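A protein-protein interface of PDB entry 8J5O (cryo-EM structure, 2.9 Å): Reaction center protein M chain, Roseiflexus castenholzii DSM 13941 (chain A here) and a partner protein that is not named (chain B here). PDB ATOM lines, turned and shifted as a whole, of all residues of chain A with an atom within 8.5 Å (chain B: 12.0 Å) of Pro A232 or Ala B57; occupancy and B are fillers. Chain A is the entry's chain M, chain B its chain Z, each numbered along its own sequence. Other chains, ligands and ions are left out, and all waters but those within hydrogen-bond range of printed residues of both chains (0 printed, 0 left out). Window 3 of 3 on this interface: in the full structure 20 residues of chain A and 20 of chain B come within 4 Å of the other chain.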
ATOM      1  N   THR A 215       9.750  19.264  -1.980  1.00  0.00           N
ATOM      2  CA  THR A 215      10.878  20.181  -2.105  1.00  0.00           C
ATOM      3  C   THR A 215      11.837  19.794  -3.226  1.00  0.00           C
ATOM      4  O   THR A 215      13.004  20.205  -3.204  1.00  0.00           O
ATOM      5  CB  THR A 215      11.631  20.274  -0.777  1.00  0.00           C
ATOM      6  OG1 THR A 215      12.087  18.971  -0.392  1.00  0.00           O
ATOM      7  CG2 THR A 215      10.732  20.829   0.311  1.00  0.00           C
ATOM      8  N   LYS A 217      11.930  20.841  -6.190  1.00  0.00           N
ATOM      9  CA  LYS A 217      12.255  21.956  -7.069  1.00  0.00           C
ATOM     10  C   LYS A 217      13.629  22.543  -6.776  1.00  0.00           C
ATOM     11  O   LYS A 217      14.165  23.281  -7.609  1.00  0.00           O
ATOM     12  CB  LYS A 217      11.186  23.041  -6.948  1.00  0.00           C
ATOM     13  CG  LYS A 217      11.259  24.116  -8.012  1.00  0.00           C
ATOM     14  CD  LYS A 217      10.600  25.395  -7.531  1.00  0.00           C
ATOM     15  CE  LYS A 217      11.274  26.620  -8.123  1.00  0.00           C
ATOM     16  NZ  LYS A 217      10.362  27.795  -8.151  1.00  0.00           N
ATOM     17  N   TRP A 218      14.209  22.234  -5.616  1.00  0.00           N
ATOM     18  CA  TRP A 218      15.539  22.701  -5.244  1.00  0.00           C
ATOM     19  C   TRP A 218      16.544  21.559  -5.157  1.00  0.00           C
ATOM     20  O   TRP A 218      17.585  21.703  -4.507  1.00  0.00           O
ATOM     21  CB  TRP A 218      15.482  23.462  -3.920  1.00  0.00           C
ATOM     22  CG  TRP A 218      14.761  24.764  -4.026  1.00  0.00           C
ATOM     23  CD1 TRP A 218      15.275  25.952  -4.453  1.00  0.00           C
ATOM     24  CD2 TRP A 218      13.388  25.010  -3.710  1.00  0.00           C
ATOM     25  NE1 TRP A 218      14.307  26.925  -4.420  1.00  0.00           N
ATOM     26  CE2 TRP A 218      13.139  26.371  -3.966  1.00  0.00           C
ATOM     27  CE3 TRP A 218      12.345  24.212  -3.232  1.00  0.00           C
ATOM     28  CZ2 TRP A 218      11.890  26.952  -3.762  1.00  0.00           C
ATOM     29  CZ3 TRP A 218      11.108  24.789  -3.028  1.00  0.00           C
ATOM     30  CH2 TRP A 218      10.891  26.146  -3.293  1.00  0.00           C
ATOM     31  N   LYS A 219      16.250  20.426  -5.796  1.00  0.00           N
ATOM     32  CA  LYS A 219      17.171  19.289  -5.863  1.00  0.00           C
ATOM     33  C   LYS A 219      17.412  18.686  -4.478  1.00  0.00           C
ATOM     34  O   LYS A 219      18.550  18.492  -4.053  1.00  0.00           O
ATOM     35  CB  LYS A 219      18.491  19.692  -6.525  1.00  0.00           C
ATOM     36  CG  LYS A 219      18.327  20.199  -7.942  1.00  0.00           C
ATOM     37  CD  LYS A 219      17.832  19.103  -8.865  1.00  0.00           C
ATOM     38  CE  LYS A 219      17.830  19.568 -10.308  1.00  0.00           C
ATOM     39  NZ  LYS A 219      16.790  20.609 -10.540  1.00  0.00           N
ATOM     40  N   SER A 220      16.321  18.388  -3.777  1.00  0.00           N
ATOM     41  CA  SER A 220      16.401  17.795  -2.450  1.00  0.00           C
ATOM     42  C   SER A 220      16.541  16.278  -2.483  1.00  0.00           C
ATOM     43  O   SER A 220      16.816  15.677  -1.440  1.00  0.00           O
ATOM     44  CB  SER A 220      15.165  18.181  -1.636  1.00  0.00           C
ATOM     45  OG  SER A 220      15.218  17.630  -0.334  1.00  0.00           O
ATOM     46  N   GLU A 226      23.593  16.318  -0.422  1.00  0.00           N
ATOM     47  CA  GLU A 226      23.099  17.095   0.712  1.00  0.00           C
ATOM     48  C   GLU A 226      23.807  16.726   2.007  1.00  0.00           C
ATOM     49  O   GLU A 226      23.861  17.540   2.933  1.00  0.00           O
ATOM     50  CB  GLU A 226      21.589  16.917   0.874  1.00  0.00           C
ATOM     51  CG  GLU A 226      20.791  17.088  -0.404  1.00  0.00           C
ATOM     52  CD  GLU A 226      20.881  18.490  -0.967  1.00  0.00           C
ATOM     53  OE1 GLU A 226      20.620  19.453  -0.216  1.00  0.00           O
ATOM     54  OE2 GLU A 226      21.214  18.630  -2.163  1.00  0.00           O
ATOM     55  N   ALA A 229      26.715  19.366   2.288  1.00  0.00           N
ATOM     56  CA  ALA A 229      26.277  20.707   2.654  1.00  0.00           C
ATOM     57  C   ALA A 229      24.789  20.836   2.367  1.00  0.00           C
ATOM     58  O   ALA A 229      24.324  20.418   1.304  1.00  0.00           O
ATOM     59  CB  ALA A 229      27.065  21.777   1.893  1.00  0.00           C
ATOM     60  N   GLU A 230      24.053  21.418   3.311  1.00  0.00           N
ATOM     61  CA  GLU A 230      22.609  21.548   3.167  1.00  0.00           C
ATOM     62  C   GLU A 230      22.256  22.570   2.094  1.00  0.00           C
ATOM     63  O   GLU A 230      22.991  23.533   1.861  1.00  0.00           O
ATOM     64  CB  GLU A 230      21.976  21.958   4.495  1.00  0.00           C
ATOM     65  CG  GLU A 230      22.230  20.994   5.637  1.00  0.00           C
ATOM     66  CD  GLU A 230      21.430  19.715   5.513  1.00  0.00           C
ATOM     67  OE1 GLU A 230      20.688  19.384   6.461  1.00  0.00           O
ATOM     68  OE2 GLU A 230      21.544  19.038   4.472  1.00  0.00           O
ATOM     69  N   GLY A 231      21.117  22.354   1.440  1.00  0.00           N
ATOM     70  CA  GLY A 231      20.625  23.262   0.434  1.00  0.00           C
ATOM     71  C   GLY A 231      19.268  23.829   0.796  1.00  0.00           C
ATOM     72  O   GLY A 231      18.718  23.547   1.865  1.00  0.00           O
ATOM     73  N   PRO A 232      18.707  24.658  -0.090  1.00  0.00           N
ATOM     74  CA  PRO A 232      17.402  25.276   0.210  1.00  0.00           C
ATOM     75  C   PRO A 232      16.272  24.278   0.417  1.00  0.00           C
ATOM     76  O   PRO A 232      15.400  24.512   1.263  1.00  0.00           O
ATOM     77  CB  PRO A 232      17.155  26.170  -1.013  1.00  0.00           C
ATOM     78  CG  PRO A 232      18.508  26.409  -1.594  1.00  0.00           C
ATOM     79  CD  PRO A 232      19.278  25.151  -1.352  1.00  0.00           C
ATOM     80  N   GLY A 233      16.256  23.173  -0.331  1.00  0.00           N
ATOM     81  CA  GLY A 233      15.184  22.202  -0.169  1.00  0.00           C
ATOM     82  C   GLY A 233      15.215  21.517   1.184  1.00  0.00           C
ATOM     83  O   GLY A 233      14.183  21.363   1.845  1.00  0.00           O
ATOM     84  N   THR A 234      16.405  21.098   1.616  1.00  0.00           N
ATOM     85  CA  THR A 234      16.544  20.484   2.932  1.00  0.00           C
ATOM     86  C   THR A 234      16.201  21.474   4.037  1.00  0.00           C
ATOM     87  O   THR A 234      15.576  21.105   5.040  1.00  0.00           O
ATOM     88  CB  THR A 234      17.963  19.944   3.110  1.00  0.00           C
ATOM     89  OG1 THR A 234      18.141  18.786   2.287  1.00  0.00           O
ATOM     90  CG2 THR A 234      18.211  19.566   4.558  1.00  0.00           C
ATOM     91  N   GLN A 235      16.604  22.735   3.871  1.00  0.00           N
ATOM     92  CA  GLN A 235      16.266  23.761   4.851  1.00  0.00           C
ATOM     93  C   GLN A 235      14.758  23.953   4.946  1.00  0.00           C
ATOM     94  O   GLN A 235      14.206  24.068   6.048  1.00  0.00           O
ATOM     95  CB  GLN A 235      16.957  25.073   4.483  1.00  0.00           C
ATOM     96  CG  GLN A 235      18.392  25.174   4.967  1.00  0.00           C
ATOM     97  CD  GLN A 235      19.242  26.076   4.094  1.00  0.00           C
ATOM     98  OE1 GLN A 235      18.785  27.116   3.623  1.00  0.00           O
ATOM     99  NE2 GLN A 235      20.490  25.680   3.875  1.00  0.00           N
ATOM    100  N   ARG A 236      14.075  23.979   3.800  1.00  0.00           N
ATOM    101  CA  ARG A 236      12.623  24.122   3.806  1.00  0.00           C
ATOM    102  C   ARG A 236      11.951  22.925   4.464  1.00  0.00           C
ATOM    103  O   ARG A 236      10.979  23.086   5.210  1.00  0.00           O
ATOM    104  CB  ARG A 236      12.110  24.307   2.380  1.00  0.00           C
ATOM    105  CG  ARG A 236      12.358  25.686   1.808  1.00  0.00           C
ATOM    106  CD  ARG A 236      11.558  25.904   0.540  1.00  0.00           C
ATOM    107  NE  ARG A 236      11.484  27.315   0.181  1.00  0.00           N
ATOM    108  CZ  ARG A 236      12.505  28.027  -0.275  1.00  0.00           C
ATOM    109  NH1 ARG A 236      13.699  27.487  -0.448  1.00  0.00           N
ATOM    110  NH2 ARG A 236      12.323  29.311  -0.563  1.00  0.00           N
ATOM    111  N   ALA A 237      12.442  21.712   4.191  1.00  0.00           N
ATOM    112  CA  ALA A 237      11.861  20.526   4.818  1.00  0.00           C
ATOM    113  C   ALA A 237      12.041  20.554   6.332  1.00  0.00           C
ATOM    114  O   ALA A 237      11.106  20.243   7.088  1.00  0.00           O
ATOM    115  CB  ALA A 237      12.484  19.263   4.227  1.00  0.00           C
ATOM    116  N   GLN A 238      13.236  20.932   6.792  1.00  0.00           N
ATOM    117  CA  GLN A 238      13.480  21.040   8.226  1.00  0.00           C
ATOM    118  C   GLN A 238      12.571  22.080   8.863  1.00  0.00           C
ATOM    119  O   GLN A 238      12.001  21.843   9.931  1.00  0.00           O
ATOM    120  CB  GLN A 238      14.944  21.387   8.485  1.00  0.00           C
ATOM    121  CG  GLN A 238      15.926  20.298   8.096  1.00  0.00           C
ATOM    122  CD  GLN A 238      17.330  20.594   8.573  1.00  0.00           C
ATOM    123  OE1 GLN A 238      18.171  19.702   8.656  1.00  0.00           O
ATOM    124  NE2 GLN A 238      17.591  21.853   8.892  1.00  0.00           N
ATOM    125  N   LEU A 239      12.416  23.237   8.216  1.00  0.00           N
ATOM    126  CA  LEU A 239      11.551  24.276   8.767  1.00  0.00           C
ATOM    127  C   LEU A 239      10.097  23.826   8.808  1.00  0.00           C
ATOM    128  O   LEU A 239       9.385  24.099   9.781  1.00  0.00           O
ATOM    129  CB  LEU A 239      11.695  25.560   7.955  1.00  0.00           C
ATOM    130  CG  LEU A 239      13.002  26.311   8.194  1.00  0.00           C
ATOM    131  CD1 LEU A 239      13.020  27.601   7.407  1.00  0.00           C
ATOM    132  CD2 LEU A 239      13.183  26.580   9.675  1.00  0.00           C
ATOM    133  N   TYR B  49      26.682  23.471  11.213  1.00  0.00           N
ATOM    134  CA  TYR B  49      27.564  22.783  10.276  1.00  0.00           C
ATOM    135  C   TYR B  49      27.478  23.497   8.930  1.00  0.00           C
ATOM    136  O   TYR B  49      26.874  24.568   8.817  1.00  0.00           O
ATOM    137  CB  TYR B  49      27.216  21.292  10.193  1.00  0.00           C
ATOM    138  CG  TYR B  49      25.748  20.972  10.000  1.00  0.00           C
ATOM    139  CD1 TYR B  49      25.109  21.219   8.794  1.00  0.00           C
ATOM    140  CD2 TYR B  49      25.005  20.407  11.026  1.00  0.00           C
ATOM    141  CE1 TYR B  49      23.775  20.921   8.619  1.00  0.00           C
ATOM    142  CE2 TYR B  49      23.671  20.108  10.860  1.00  0.00           C
ATOM    143  CZ  TYR B  49      23.060  20.366   9.654  1.00  0.00           C
ATOM    144  OH  TYR B  49      21.730  20.069   9.483  1.00  0.00           O
ATOM    145  N   LEU B  50      28.091  22.903   7.905  1.00  0.00           N
ATOM    146  CA  LEU B  50      28.118  23.530   6.589  1.00  0.00           C
ATOM    147  C   LEU B  50      26.717  23.662   6.005  1.00  0.00           C
ATOM    148  O   LEU B  50      25.911  22.730   6.052  1.00  0.00           O
ATOM    149  CB  LEU B  50      29.004  22.736   5.627  1.00  0.00           C
ATOM    150  CG  LEU B  50      30.523  22.883   5.735  1.00  0.00           C
ATOM    151  CD1 LEU B  50      31.068  22.216   6.977  1.00  0.00           C
ATOM    152  CD2 LEU B  50      31.187  22.323   4.489  1.00  0.00           C
ATOM    153  N   ARG B  51      26.438  24.836   5.446  1.00  0.00           N
ATOM    154  CA  ARG B  51      25.174  25.106   4.778  1.00  0.00           C
ATOM    155  C   ARG B  51      25.420  26.128   3.681  1.00  0.00           C
ATOM    156  O   ARG B  51      26.403  26.871   3.707  1.00  0.00           O
ATOM    157  CB  ARG B  51      24.111  25.622   5.756  1.00  0.00           C
ATOM    158  CG  ARG B  51      23.474  24.554   6.628  1.00  0.00           C
ATOM    159  CD  ARG B  51      23.110  25.112   7.996  1.00  0.00           C
ATOM    160  NE  ARG B  51      22.233  24.225   8.748  1.00  0.00           N
ATOM    161  CZ  ARG B  51      22.373  23.952  10.038  1.00  0.00           C
ATOM    162  NH1 ARG B  51      23.358  24.469  10.751  1.00  0.00           N
ATOM    163  NH2 ARG B  51      21.503  23.137  10.628  1.00  0.00           N
ATOM    164  N   LEU B  52      24.513  26.159   2.710  1.00  0.00           N
ATOM    165  CA  LEU B  52      24.551  27.162   1.657  1.00  0.00           C
ATOM    166  C   LEU B  52      23.782  28.394   2.116  1.00  0.00           C
ATOM    167  O   LEU B  52      22.697  28.275   2.694  1.00  0.00           O
ATOM    168  CB  LEU B  52      23.960  26.612   0.359  1.00  0.00           C
ATOM    169  CG  LEU B  52      24.739  25.473  -0.300  1.00  0.00           C
ATOM    170  CD1 LEU B  52      23.982  24.926  -1.496  1.00  0.00           C
ATOM    171  CD2 LEU B  52      26.128  25.935  -0.711  1.00  0.00           C
ATOM    172  N   ASP B  53      24.346  29.567   1.867  1.00  0.00           N
ATOM    173  CA  ASP B  53      23.755  30.807   2.345  1.00  0.00           C
ATOM    174  C   ASP B  53      22.408  31.044   1.670  1.00  0.00           C
ATOM    175  O   ASP B  53      22.344  31.087   0.433  1.00  0.00           O
ATOM    176  CB  ASP B  53      24.701  31.973   2.076  1.00  0.00           C
ATOM    177  CG  ASP B  53      24.210  33.274   2.673  1.00  0.00           C
ATOM    178  OD1 ASP B  53      24.294  33.431   3.909  1.00  0.00           O
ATOM    179  OD2 ASP B  53      23.747  34.142   1.906  1.00  0.00           O
ATOM    180  N   PRO B  54      21.317  31.186   2.429  1.00  0.00           N
ATOM    181  CA  PRO B  54      20.007  31.404   1.793  1.00  0.00           C
ATOM    182  C   PRO B  54      19.925  32.688   0.990  1.00  0.00           C
ATOM    183  O   PRO B  54      19.174  32.747   0.008  1.00  0.00           O
ATOM    184  CB  PRO B  54      19.037  31.416   2.984  1.00  0.00           C
ATOM    185  CG  PRO B  54      19.884  31.720   4.173  1.00  0.00           C
ATOM    186  CD  PRO B  54      21.218  31.108   3.895  1.00  0.00           C
ATOM    187  N   ALA B  55      20.664  33.729   1.383  1.00  0.00           N
ATOM    188  CA  ALA B  55      20.633  34.977   0.627  1.00  0.00           C
ATOM    189  C   ALA B  55      21.198  34.789  -0.774  1.00  0.00           C
ATOM    190  O   ALA B  55      20.617  35.269  -1.755  1.00  0.00           O
ATOM    191  CB  ALA B  55      21.403  36.061   1.378  1.00  0.00           C
ATOM    192  N   LYS B  56      22.336  34.102  -0.891  1.00  0.00           N
ATOM    193  CA  LYS B  56      22.896  33.826  -2.209  1.00  0.00           C
ATOM    194  C   LYS B  56      22.164  32.681  -2.899  1.00  0.00           C
ATOM    195  O   LYS B  56      21.975  32.704  -4.120  1.00  0.00           O
ATOM    196  CB  LYS B  56      24.391  33.522  -2.093  1.00  0.00           C
ATOM    197  CG  LYS B  56      24.717  32.223  -1.377  1.00  0.00           C
ATOM    198  CD  LYS B  56      26.218  32.001  -1.284  1.00  0.00           C
ATOM    199  CE  LYS B  56      26.543  30.719  -0.528  1.00  0.00           C
ATOM    200  NZ  LYS B  56      26.101  29.510  -1.272  1.00  0.00           N
ATOM    201  N   ALA B  57      21.743  31.674  -2.137  1.00  0.00           N
ATOM    202  CA  ALA B  57      21.119  30.494  -2.715  1.00  0.00           C
ATOM    203  C   ALA B  57      19.670  30.775  -3.090  1.00  0.00           C
ATOM    204  O   ALA B  57      18.911  31.355  -2.308  1.00  0.00           O
ATOM    205  CB  ALA B  57      21.186  29.320  -1.740  1.00  0.00           C
ATOM    206  N   ASN B  58      19.291  30.353  -4.290  1.00  0.00           N
ATOM    207  CA  ASN B  58      17.935  30.555  -4.780  1.00  0.00           C
ATOM    208  C   ASN B  58      17.429  29.308  -5.499  1.00  0.00           C
ATOM    209  O   ASN B  58      16.272  28.917  -5.346  1.00  0.00           O
ATOM    210  CB  ASN B  58      17.879  31.764  -5.716  1.00  0.00           C
ATOM    211  CG  ASN B  58      17.800  33.080  -4.965  1.00  0.00           C
ATOM    212  OD1 ASN B  58      17.143  33.179  -3.929  1.00  0.00           O
ATOM    213  ND2 ASN B  58      18.475  34.099  -5.486  1.00  0.00           N
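NE1 of Trp A218 lies within hydrogen-bond range of O of Asn B58 (2.9 Å). The side-chain carboxylate of Glu A230 lies within hydrogen-bond range of the side-chain hydroxyl of Tyr B49, 3.3 Å away. O of Glu A230 is in hydrogen-bond range of N of Leu B52 (3.2 Å).
OE1 of Glu A230 sits close to OE1 of Gln A238, 3.4 Å away. NE2 of Gln A235 lies close to O of Gly A231 (3.4 Å). OH of Tyr B49 lies within hydrogen-bond range of NH2 of Arg B51, at 3.3 Å.
Leu B50 touches Ala A229 (O to CA, 3.97 Å). O of Leu B50 touches N of Glu A230, at 3.6 Å. CG of Arg B51 touches CB of Glu A230, 3.7 Å away. CB of Ala B57 touches CG of Pro A232, at 3.96 Å. Gln A235 touches Leu B52 (NE2 to O, 3.6 Å). OH of Tyr B49 touches OE1 of Gln A238, 3.7 Å away.
Of chain B, only Asn B58 (2.9 Å) comes within 4 Å of Trp A218. No residue of chain B comes within 4 Å of Gly A231. No residue of chain B comes within 4 Å of Thr A234. No residue of chain B comes within 4 Å of Arg A236. Of the printed residues of chain B, Ala A229 touches Leu B50 (3.97 Å). Of the printed residues of chain A, Arg B51 touches Glu A230 (3.7 Å). Of the printed residues of chain A, Leu B52 touches Glu A230 and Gln A235. Of the printed residues of chain A, Asn B58 touches Trp A218. Of the printed residues of chain B, Glu A230 touches Tyr B49 (3.3 Å), Leu B50 (3.6 Å), Arg B51 (3.7 Å) and Leu B52 (3.2 Å). Leu A239 touches none of the printed residues of chain B. The nearest residue of chain B that does not touch Pro A232 is Leu B52 (4.7 Å). The nearest printed residue of chain B that does not touch Glu A230 is Asp B53 (6.2 Å).
Hydrophobic or aromatic side chains of chain B within 4 Å of the printed part of chain A: Tyr B49, Leu B52 and Ala B57. Of the 17 printed residues of chain A, 6 touch a printed residue of chain B.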
